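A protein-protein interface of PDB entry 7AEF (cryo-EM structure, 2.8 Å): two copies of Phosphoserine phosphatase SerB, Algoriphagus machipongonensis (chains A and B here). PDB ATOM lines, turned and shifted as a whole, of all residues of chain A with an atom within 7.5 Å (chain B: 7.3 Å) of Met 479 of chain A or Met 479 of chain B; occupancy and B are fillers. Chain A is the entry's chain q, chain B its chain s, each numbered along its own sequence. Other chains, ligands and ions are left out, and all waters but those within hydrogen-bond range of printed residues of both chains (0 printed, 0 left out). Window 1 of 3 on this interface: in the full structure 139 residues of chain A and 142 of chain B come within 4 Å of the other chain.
Among the printed residues, merely in contact across the chains: Lys 469 of chain A with Thr 473 of chain B, Met 479 of chain A with Met 479 of chain B and Leu 488 of chain A with Ile 490 of chain B.
O of Ile 471 of chain B is in hydrogen-bond range of N of Met 479 of chain B (2.9 Å). The backbone NH of Met 479 of chain A is in hydrogen-bond range of the backbone carbonyl oxygen of Ile 471 of chain A (2.9 Å). The backbone NH of Phe 481 of chain A is in hydrogen-bond range of the backbone carbonyl oxygen of Lys 469 of chain A (2.8 Å).
Lys 469 of chain A touches Thr 473 of chain B, but with the chains exchanged Thr 473 of chain A does not touch Lys 469 of chain B (19.5 Å). Met 479 of chain A touches its own counterpart, Met 479 of chain B. Leu 488 of chain A touches Ile 490 of chain B, but with the chains exchanged Ile 490 of chain A does not touch Leu 488 of chain B (8.8 Å). Of the 3 pairs that touch across the chains among the printed residues, 1 has its exchanged pair printed and touching as well.
Printed residues of chain B that touch a printed residue of chain A: Thr 473, Met 479 and Ile 490. Of the 16 printed residues of chain A, 3 touch a printed residue of chain B. Among the printed residues, 3 pairs touch across the chains. Among the printed residues, no Asp or Glu carboxylate lies within 4 Å of a Lys or Arg side-chain nitrogen of the other chain.
Printed residues of chain B within 4 Å of Lys 469 of chain A: Thr 473 (3.8 Å). Of chain B, only Met 479 comes within 4 Å of Met 479 of chain A. Printed residues of chain B within 4 Å of Leu 488 of chain A: Ile 490 (3.6 Å). Of chain A, only Met 479 comes within 4 Å of Met 479 of chain B. Of the printed residues of chain A, Ile 490 of chain B touches Leu 488. The nearest residue of chain B that does not touch Met 479 of chain A is Ile 490 of chain B (5.4 Å). The nearest residue of chain A that does not touch Met 479 of chain B is Phe 481 of chain A (5.1 Å). The nearest printed residue of chain B that does not touch Leu 488 of chain A is Ile 477 of chain B (4.9 Å).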
ATOM      1  N   ILE A 460       5.435   0.186   1.148  1.00  0.00           N
ATOM      2  CA  ILE A 460       5.900   1.060   0.076  1.00  0.00           C
ATOM      3  C   ILE A 460       6.672   2.240   0.651  1.00  0.00           C
ATOM      4  O   ILE A 460       6.118   3.076   1.354  1.00  0.00           O
ATOM      5  CB  ILE A 460       4.744   1.554  -0.819  1.00  0.00           C
ATOM      6  CG1 ILE A 460       4.045   0.335  -1.492  1.00  0.00           C
ATOM      7  CG2 ILE A 460       5.275   2.544  -1.861  1.00  0.00           C
ATOM      8  CD1 ILE A 460       2.758   0.650  -2.251  1.00  0.00           C
ATOM      9  N   LYS A 469       2.149   3.299  -5.870  1.00  0.00           N
ATOM     10  CA  LYS A 469       0.913   3.084  -5.106  1.00  0.00           C
ATOM     11  C   LYS A 469       0.366   1.675  -5.267  1.00  0.00           C
ATOM     12  O   LYS A 469       0.538   1.069  -6.318  1.00  0.00           O
ATOM     13  CB  LYS A 469      -0.173   4.043  -5.556  1.00  0.00           C
ATOM     14  CG  LYS A 469       0.120   5.489  -5.310  1.00  0.00           C
ATOM     15  CD  LYS A 469      -0.998   6.378  -5.831  1.00  0.00           C
ATOM     16  CE  LYS A 469      -0.859   6.670  -7.316  1.00  0.00           C
ATOM     17  NZ  LYS A 469       0.221   7.611  -7.554  1.00  0.00           N
ATOM     18  N   GLY A 470      -0.368   1.162  -4.289  1.00  0.00           N
ATOM     19  CA  GLY A 470      -0.984  -0.134  -4.540  1.00  0.00           C
ATOM     20  C   GLY A 470      -1.461  -0.905  -3.325  1.00  0.00           C
ATOM     21  O   GLY A 470      -1.563  -0.377  -2.220  1.00  0.00           O
ATOM     22  N   ILE A 471      -1.774  -2.168  -3.583  1.00  0.00           N
ATOM     23  CA  ILE A 471      -2.296  -3.133  -2.628  1.00  0.00           C
ATOM     24  C   ILE A 471      -1.359  -4.320  -2.444  1.00  0.00           C
ATOM     25  O   ILE A 471      -0.877  -4.906  -3.412  1.00  0.00           O
ATOM     26  CB  ILE A 471      -3.667  -3.667  -3.096  1.00  0.00           C
ATOM     27  CG1 ILE A 471      -4.657  -2.511  -3.205  1.00  0.00           C
ATOM     28  CG2 ILE A 471      -4.185  -4.758  -2.134  1.00  0.00           C
ATOM     29  CD1 ILE A 471      -5.939  -2.849  -3.915  1.00  0.00           C
ATOM     30  N   GLN A 472      -1.093  -4.678  -1.199  1.00  0.00           N
ATOM     31  CA  GLN A 472      -0.290  -5.851  -0.896  1.00  0.00           C
ATOM     32  C   GLN A 472      -0.910  -6.584   0.267  1.00  0.00           C
ATOM     33  O   GLN A 472      -1.120  -5.987   1.321  1.00  0.00           O
ATOM     34  CB  GLN A 472       1.145  -5.480  -0.568  1.00  0.00           C
ATOM     35  CG  GLN A 472       2.021  -6.679  -0.260  1.00  0.00           C
ATOM     36  CD  GLN A 472       3.437  -6.302  -0.061  1.00  0.00           C
ATOM     37  OE1 GLN A 472       3.923  -5.354  -0.675  1.00  0.00           O
ATOM     38  NE2 GLN A 472       4.135  -7.023   0.793  1.00  0.00           N
ATOM     39  N   THR A 473      -1.255  -7.852   0.105  1.00  0.00           N
ATOM     40  CA  THR A 473      -1.878  -8.620   1.186  1.00  0.00           C
ATOM     41  C   THR A 473      -0.916  -9.387   2.083  1.00  0.00           C
ATOM     42  O   THR A 473       0.281  -9.271   1.963  1.00  0.00           O
ATOM     43  CB  THR A 473      -3.064  -9.516   0.726  1.00  0.00           C
ATOM     44  OG1 THR A 473      -2.587 -10.622  -0.021  1.00  0.00           O
ATOM     45  CG2 THR A 473      -4.077  -8.767  -0.098  1.00  0.00           C
ATOM     46  N   GLY A 476       1.300 -12.107   0.359  1.00  0.00           N
ATOM     47  CA  GLY A 476       2.190 -11.628  -0.685  1.00  0.00           C
ATOM     48  C   GLY A 476       1.578 -11.350  -2.064  1.00  0.00           C
ATOM     49  O   GLY A 476       2.324 -11.154  -3.019  1.00  0.00           O
ATOM     50  N   ILE A 477       0.258 -11.343  -2.211  1.00  0.00           N
ATOM     51  CA  ILE A 477      -0.313 -11.034  -3.519  1.00  0.00           C
ATOM     52  C   ILE A 477      -0.294  -9.529  -3.681  1.00  0.00           C
ATOM     53  O   ILE A 477      -0.731  -8.795  -2.788  1.00  0.00           O
ATOM     54  CB  ILE A 477      -1.756 -11.547  -3.690  1.00  0.00           C
ATOM     55  CG1 ILE A 477      -1.774 -13.055  -3.570  1.00  0.00           C
ATOM     56  CG2 ILE A 477      -2.297 -11.096  -5.071  1.00  0.00           C
ATOM     57  CD1 ILE A 477      -3.133 -13.644  -3.417  1.00  0.00           C
ATOM     58  N   LYS A 478       0.248  -9.064  -4.797  1.00  0.00           N
ATOM     59  CA  LYS A 478       0.371  -7.643  -5.060  1.00  0.00           C
ATOM     60  C   LYS A 478      -0.399  -7.131  -6.262  1.00  0.00           C
ATOM     61  O   LYS A 478      -0.574  -7.821  -7.272  1.00  0.00           O
ATOM     62  CB  LYS A 478       1.825  -7.306  -5.315  1.00  0.00           C
ATOM     63  CG  LYS A 478       2.740  -7.516  -4.184  1.00  0.00           C
ATOM     64  CD  LYS A 478       4.139  -7.156  -4.595  1.00  0.00           C
ATOM     65  CE  LYS A 478       5.114  -7.385  -3.485  1.00  0.00           C
ATOM     66  NZ  LYS A 478       6.501  -7.039  -3.890  1.00  0.00           N
ATOM     67  N   MET A 479      -0.743  -5.857  -6.192  1.00  0.00           N
ATOM     68  CA  MET A 479      -1.258  -5.108  -7.326  1.00  0.00           C
ATOM     69  C   MET A 479      -0.699  -3.703  -7.223  1.00  0.00           C
ATOM     70  O   MET A 479      -1.102  -2.903  -6.374  1.00  0.00           O
ATOM     71  CB  MET A 479      -2.766  -5.126  -7.334  1.00  0.00           C
ATOM     72  CG  MET A 479      -3.369  -4.375  -8.454  1.00  0.00           C
ATOM     73  SD  MET A 479      -5.115  -4.596  -8.531  1.00  0.00           S
ATOM     74  CE  MET A 479      -5.461  -3.674 -10.014  1.00  0.00           C
ATOM     75  N   ILE A 480       0.250  -3.402  -8.102  1.00  0.00           N
ATOM     76  CA  ILE A 480       0.987  -2.150  -8.005  1.00  0.00           C
ATOM     77  C   ILE A 480       0.891  -1.254  -9.221  1.00  0.00           C
ATOM     78  O   ILE A 480       1.025  -1.690 -10.366  1.00  0.00           O
ATOM     79  CB  ILE A 480       2.472  -2.431  -7.687  1.00  0.00           C
ATOM     80  CG1 ILE A 480       2.605  -3.335  -6.400  1.00  0.00           C
ATOM     81  CG2 ILE A 480       3.267  -1.112  -7.509  1.00  0.00           C
ATOM     82  CD1 ILE A 480       2.083  -2.768  -5.065  1.00  0.00           C
ATOM     83  N   PHE A 481       0.683   0.020  -8.944  1.00  0.00           N
ATOM     84  CA  PHE A 481       0.594   1.067  -9.936  1.00  0.00           C
ATOM     85  C   PHE A 481       1.834   1.960  -9.908  1.00  0.00           C
ATOM     86  O   PHE A 481       2.119   2.634  -8.913  1.00  0.00           O
ATOM     87  CB  PHE A 481      -0.598   1.962  -9.626  1.00  0.00           C
ATOM     88  CG  PHE A 481      -1.929   1.320  -9.695  1.00  0.00           C
ATOM     89  CD1 PHE A 481      -2.412   0.609  -8.622  1.00  0.00           C
ATOM     90  CD2 PHE A 481      -2.720   1.454 -10.800  1.00  0.00           C
ATOM     91  CE1 PHE A 481      -3.643   0.034  -8.658  1.00  0.00           C
ATOM     92  CE2 PHE A 481      -3.964   0.887 -10.837  1.00  0.00           C
ATOM     93  CZ  PHE A 481      -4.422   0.177  -9.766  1.00  0.00           C
ATOM     94  N   LEU A 488       1.147  -1.186 -14.816  1.00  0.00           N
ATOM     95  CA  LEU A 488       0.284  -1.903 -13.875  1.00  0.00           C
ATOM     96  C   LEU A 488       0.654  -3.367 -13.794  1.00  0.00           C
ATOM     97  O   LEU A 488       0.598  -4.109 -14.779  1.00  0.00           O
ATOM     98  CB  LEU A 488      -1.209  -1.787 -14.186  1.00  0.00           C
ATOM     99  CG  LEU A 488      -2.167  -2.688 -13.269  1.00  0.00           C
ATOM    100  CD1 LEU A 488      -2.074  -2.297 -11.785  1.00  0.00           C
ATOM    101  CD2 LEU A 488      -3.574  -2.517 -13.733  1.00  0.00           C
ATOM    102  N   GLN A 489       1.031  -3.802 -12.607  1.00  0.00           N
ATOM    103  CA  GLN A 489       1.441  -5.184 -12.454  1.00  0.00           C
ATOM    104  C   GLN A 489       0.728  -5.951 -11.355  1.00  0.00           C
ATOM    105  O   GLN A 489       0.702  -5.547 -10.189  1.00  0.00           O
ATOM    106  CB  GLN A 489       2.937  -5.230 -12.244  1.00  0.00           C
ATOM    107  CG  GLN A 489       3.514  -6.605 -12.099  1.00  0.00           C
ATOM    108  CD  GLN A 489       4.995  -6.543 -12.116  1.00  0.00           C
ATOM    109  OE1 GLN A 489       5.557  -5.611 -12.697  1.00  0.00           O
ATOM    110  NE2 GLN A 489       5.667  -7.488 -11.489  1.00  0.00           N
ATOM    111  N   ILE A 490       0.161  -7.089 -11.745  1.00  0.00           N
ATOM    112  CA  ILE A 490      -0.548  -7.986 -10.837  1.00  0.00           C
ATOM    113  C   ILE A 490       0.254  -9.263 -10.682  1.00  0.00           C
ATOM    114  O   ILE A 490       0.560  -9.929 -11.670  1.00  0.00           O
ATOM    115  CB  ILE A 490      -1.958  -8.286 -11.349  1.00  0.00           C
ATOM    116  CG1 ILE A 490      -2.736  -6.964 -11.455  1.00  0.00           C
ATOM    117  CG2 ILE A 490      -2.637  -9.251 -10.385  1.00  0.00           C
ATOM    118  CD1 ILE A 490      -4.036  -7.036 -12.193  1.00  0.00           C
ATOM    119  N   GLU A 491       0.610  -9.609  -9.453  1.00  0.00           N
ATOM    120  CA  GLU A 491       1.488 -10.761  -9.240  1.00  0.00           C
ATOM    121  C   GLU A 491       1.292 -11.549  -7.950  1.00  0.00           C
ATOM    122  O   GLU A 491       1.157 -10.972  -6.868  1.00  0.00           O
ATOM    123  CB  GLU A 491       2.926 -10.255  -9.311  1.00  0.00           C
ATOM    124  CG  GLU A 491       3.978 -11.293  -9.093  1.00  0.00           C
ATOM    125  CD  GLU A 491       5.343 -10.771  -9.297  1.00  0.00           C
ATOM    126  OE1 GLU A 491       5.483  -9.677  -9.786  1.00  0.00           O
ATOM    127  OE2 GLU A 491       6.272 -11.457  -8.950  1.00  0.00           O
ATOM    128  N   ILE B 460     -15.135  11.607 -11.404  1.00  0.00           N
ATOM    129  CA  ILE B 460     -16.370  10.931 -11.789  1.00  0.00           C
ATOM    130  C   ILE B 460     -17.574  11.803 -11.467  1.00  0.00           C
ATOM    131  O   ILE B 460     -17.861  12.085 -10.308  1.00  0.00           O
ATOM    132  CB  ILE B 460     -16.511   9.546 -11.121  1.00  0.00           C
ATOM    133  CG1 ILE B 460     -15.331   8.629 -11.563  1.00  0.00           C
ATOM    134  CG2 ILE B 460     -17.866   8.928 -11.478  1.00  0.00           C
ATOM    135  CD1 ILE B 460     -15.224   7.294 -10.828  1.00  0.00           C
ATOM    136  N   LYS B 469     -18.163   3.854 -10.714  1.00  0.00           N
ATOM    137  CA  LYS B 469     -17.228   3.845  -9.581  1.00  0.00           C
ATOM    138  C   LYS B 469     -15.820   3.446  -9.990  1.00  0.00           C
ATOM    139  O   LYS B 469     -15.650   2.663 -10.916  1.00  0.00           O
ATOM    140  CB  LYS B 469     -17.682   2.864  -8.515  1.00  0.00           C
ATOM    141  CG  LYS B 469     -18.987   3.197  -7.864  1.00  0.00           C
ATOM    142  CD  LYS B 469     -19.386   2.141  -6.848  1.00  0.00           C
ATOM    143  CE  LYS B 469     -20.084   0.954  -7.490  1.00  0.00           C
ATOM    144  NZ  LYS B 469     -21.433   1.309  -7.891  1.00  0.00           N
ATOM    145  N   GLY B 470     -14.799   3.890  -9.270  1.00  0.00           N
ATOM    146  CA  GLY B 470     -13.481   3.377  -9.614  1.00  0.00           C
ATOM    147  C   GLY B 470     -12.291   4.166  -9.102  1.00  0.00           C
ATOM    148  O   GLY B 470     -12.410   5.034  -8.240  1.00  0.00           O
ATOM    149  N   ILE B 471     -11.136   3.807  -9.649  1.00  0.00           N
ATOM    150  CA  ILE B 471      -9.828   4.356  -9.326  1.00  0.00           C
ATOM    151  C   ILE B 471      -9.181   5.036 -10.526  1.00  0.00           C
ATOM    152  O   ILE B 471      -9.146   4.488 -11.625  1.00  0.00           O
ATOM    153  CB  ILE B 471      -8.881   3.239  -8.835  1.00  0.00           C
ATOM    154  CG1 ILE B 471      -9.459   2.595  -7.579  1.00  0.00           C
ATOM    155  CG2 ILE B 471      -7.465   3.799  -8.577  1.00  0.00           C
ATOM    156  CD1 ILE B 471      -8.782   1.317  -7.162  1.00  0.00           C
ATOM    157  N   GLN B 472      -8.670   6.238 -10.319  1.00  0.00           N
ATOM    158  CA  GLN B 472      -7.944   6.948 -11.361  1.00  0.00           C
ATOM    159  C   GLN B 472      -6.737   7.615 -10.749  1.00  0.00           C
ATOM    160  O   GLN B 472      -6.880   8.382  -9.800  1.00  0.00           O
ATOM    161  CB  GLN B 472      -8.817   7.984 -12.046  1.00  0.00           C
ATOM    162  CG  GLN B 472      -8.101   8.737 -13.151  1.00  0.00           C
ATOM    163  CD  GLN B 472      -9.002   9.653 -13.880  1.00  0.00           C
ATOM    164  OE1 GLN B 472     -10.191   9.375 -14.027  1.00  0.00           O
ATOM    165  NE2 GLN B 472      -8.475  10.764 -14.356  1.00  0.00           N
ATOM    166  N   THR B 473      -5.540   7.322 -11.233  1.00  0.00           N
ATOM    167  CA  THR B 473      -4.323   7.920 -10.676  1.00  0.00           C
ATOM    168  C   THR B 473      -3.862   9.206 -11.345  1.00  0.00           C
ATOM    169  O   THR B 473      -4.527   9.742 -12.200  1.00  0.00           O
ATOM    170  CB  THR B 473      -3.146   6.916 -10.502  1.00  0.00           C
ATOM    171  OG1 THR B 473      -2.607   6.563 -11.764  1.00  0.00           O
ATOM    172  CG2 THR B 473      -3.551   5.662  -9.773  1.00  0.00           C
ATOM    173  N   GLY B 476      -2.969   8.990 -15.144  1.00  0.00           N
ATOM    174  CA  GLY B 476      -4.047   8.574 -16.023  1.00  0.00           C
ATOM    175  C   GLY B 476      -4.373   7.075 -16.085  1.00  0.00           C
ATOM    176  O   GLY B 476      -5.122   6.663 -16.964  1.00  0.00           O
ATOM    177  N   ILE B 477      -3.828   6.245 -15.201  1.00  0.00           N
ATOM    178  CA  ILE B 477      -4.179   4.829 -15.243  1.00  0.00           C
ATOM    179  C   ILE B 477      -5.518   4.670 -14.556  1.00  0.00           C
ATOM    180  O   ILE B 477      -5.720   5.176 -13.445  1.00  0.00           O
ATOM    181  CB  ILE B 477      -3.140   3.925 -14.550  1.00  0.00           C
ATOM    182  CG1 ILE B 477      -1.809   4.049 -15.259  1.00  0.00           C
ATOM    183  CG2 ILE B 477      -3.644   2.459 -14.574  1.00  0.00           C
ATOM    184  CD1 ILE B 477      -0.659   3.465 -14.515  1.00  0.00           C
ATOM    185  N   LYS B 478      -6.447   4.007 -15.227  1.00  0.00           N
ATOM    186  CA  LYS B 478      -7.788   3.819 -14.703  1.00  0.00           C
ATOM    187  C   LYS B 478      -8.196   2.381 -14.447  1.00  0.00           C
ATOM    188  O   LYS B 478      -7.790   1.449 -15.148  1.00  0.00           O
ATOM    189  CB  LYS B 478      -8.791   4.374 -15.692  1.00  0.00           C
ATOM    190  CG  LYS B 478      -8.725   5.823 -15.931  1.00  0.00           C
ATOM    191  CD  LYS B 478      -9.765   6.215 -16.942  1.00  0.00           C
ATOM    192  CE  LYS B 478      -9.714   7.680 -17.242  1.00  0.00           C
ATOM    193  NZ  LYS B 478     -10.734   8.070 -18.250  1.00  0.00           N
ATOM    194  N   MET B 479      -9.117   2.230 -13.510  1.00  0.00           N
ATOM    195  CA  MET B 479      -9.823   0.981 -13.283  1.00  0.00           C
ATOM    196  C   MET B 479     -11.249   1.338 -12.912  1.00  0.00           C
ATOM    197  O   MET B 479     -11.534   1.822 -11.813  1.00  0.00           O
ATOM    198  CB  MET B 479      -9.137   0.169 -12.214  1.00  0.00           C
ATOM    199  CG  MET B 479      -9.803  -1.115 -11.914  1.00  0.00           C
ATOM    200  SD  MET B 479      -8.856  -2.108 -10.810  1.00  0.00           S
ATOM    201  CE  MET B 479      -9.877  -3.566 -10.779  1.00  0.00           C
ATOM    202  N   ILE B 480     -12.159   1.095 -13.849  1.00  0.00           N
ATOM    203  CA  ILE B 480     -13.534   1.544 -13.686  1.00  0.00           C
ATOM    204  C   ILE B 480     -14.576   0.446 -13.723  1.00  0.00           C
ATOM    205  O   ILE B 480     -14.559  -0.440 -14.580  1.00  0.00           O
ATOM    206  CB  ILE B 480     -13.873   2.612 -14.750  1.00  0.00           C
ATOM    207  CG1 ILE B 480     -12.823   3.790 -14.712  1.00  0.00           C
ATOM    208  CG2 ILE B 480     -15.310   3.160 -14.557  1.00  0.00           C
ATOM    209  CD1 ILE B 480     -12.727   4.627 -13.421  1.00  0.00           C
ATOM    210  N   PHE B 481     -15.502   0.542 -12.788  1.00  0.00           N
ATOM    211  CA  PHE B 481     -16.617  -0.365 -12.646  1.00  0.00           C
ATOM    212  C   PHE B 481     -17.927   0.301 -13.063  1.00  0.00           C
ATOM    213  O   PHE B 481     -18.371   1.280 -12.456  1.00  0.00           O
ATOM    214  CB  PHE B 481     -16.770  -0.758 -11.183  1.00  0.00           C
ATOM    215  CG  PHE B 481     -15.645  -1.514 -10.591  1.00  0.00           C
ATOM    216  CD1 PHE B 481     -14.541  -0.851 -10.111  1.00  0.00           C
ATOM    217  CD2 PHE B 481     -15.695  -2.874 -10.470  1.00  0.00           C
ATOM    218  CE1 PHE B 481     -13.510  -1.526  -9.538  1.00  0.00           C
ATOM    219  CE2 PHE B 481     -14.664  -3.557  -9.886  1.00  0.00           C
ATOM    220  CZ  PHE B 481     -13.574  -2.883  -9.423  1.00  0.00           C
ATOM    221  N   LEU B 488     -16.205  -4.148 -16.483  1.00  0.00           N
ATOM    222  CA  LEU B 488     -14.960  -3.798 -15.794  1.00  0.00           C
ATOM    223  C   LEU B 488     -13.851  -3.501 -16.777  1.00  0.00           C
ATOM    224  O   LEU B 488     -13.446  -4.347 -17.580  1.00  0.00           O
ATOM    225  CB  LEU B 488     -14.475  -4.860 -14.807  1.00  0.00           C
ATOM    226  CG  LEU B 488     -13.037  -4.578 -14.156  1.00  0.00           C
ATOM    227  CD1 LEU B 488     -13.028  -3.282 -13.329  1.00  0.00           C
ATOM    228  CD2 LEU B 488     -12.677  -5.725 -13.273  1.00  0.00           C
ATOM    229  N   GLN B 489     -13.338  -2.288 -16.719  1.00  0.00           N
ATOM    230  CA  GLN B 489     -12.296  -1.910 -17.654  1.00  0.00           C
ATOM    231  C   GLN B 489     -11.035  -1.345 -17.025  1.00  0.00           C
ATOM    232  O   GLN B 489     -11.066  -0.382 -16.254  1.00  0.00           O
ATOM    233  CB  GLN B 489     -12.870  -0.932 -18.655  1.00  0.00           C
ATOM    234  CG  GLN B 489     -11.911  -0.473 -19.711  1.00  0.00           C
ATOM    235  CD  GLN B 489     -12.629   0.303 -20.750  1.00  0.00           C
ATOM    236  OE1 GLN B 489     -13.830   0.091 -20.944  1.00  0.00           O
ATOM    237  NE2 GLN B 489     -11.956   1.211 -21.428  1.00  0.00           N
ATOM    238  N   ILE B 490      -9.910  -1.954 -17.387  1.00  0.00           N
ATOM    239  CA  ILE B 490      -8.589  -1.547 -16.917  1.00  0.00           C
ATOM    240  C   ILE B 490      -7.812  -0.959 -18.080  1.00  0.00           C
ATOM    241  O   ILE B 490      -7.636  -1.617 -19.105  1.00  0.00           O
ATOM    242  CB  ILE B 490      -7.837  -2.725 -16.298  1.00  0.00           C
ATOM    243  CG1 ILE B 490      -8.649  -3.258 -15.106  1.00  0.00           C
ATOM    244  CG2 ILE B 490      -6.457  -2.252 -15.857  1.00  0.00           C
ATOM    245  CD1 ILE B 490      -8.200  -4.576 -14.554  1.00  0.00           C
ATOM    246  N   GLU B 491      -7.355   0.277 -17.940  1.00  0.00           N
ATOM    247  CA  GLU B 491      -6.705   0.949 -19.066  1.00  0.00           C
ATOM    248  C   GLU B 491      -5.606   1.952 -18.730  1.00  0.00           C
ATOM    249  O   GLU B 491      -5.758   2.782 -17.830  1.00  0.00           O
ATOM    250  CB  GLU B 491      -7.797   1.647 -19.870  1.00  0.00           C
ATOM    251  CG  GLU B 491      -7.321   2.415 -21.060  1.00  0.00           C
ATOM    252  CD  GLU B 491      -8.430   2.961 -21.866  1.00  0.00           C
ATOM    253  OE1 GLU B 491      -9.556   2.599 -21.630  1.00  0.00           O
ATOM    254  OE2 GLU B 491      -8.166   3.765 -22.725  1.00  0.00           O
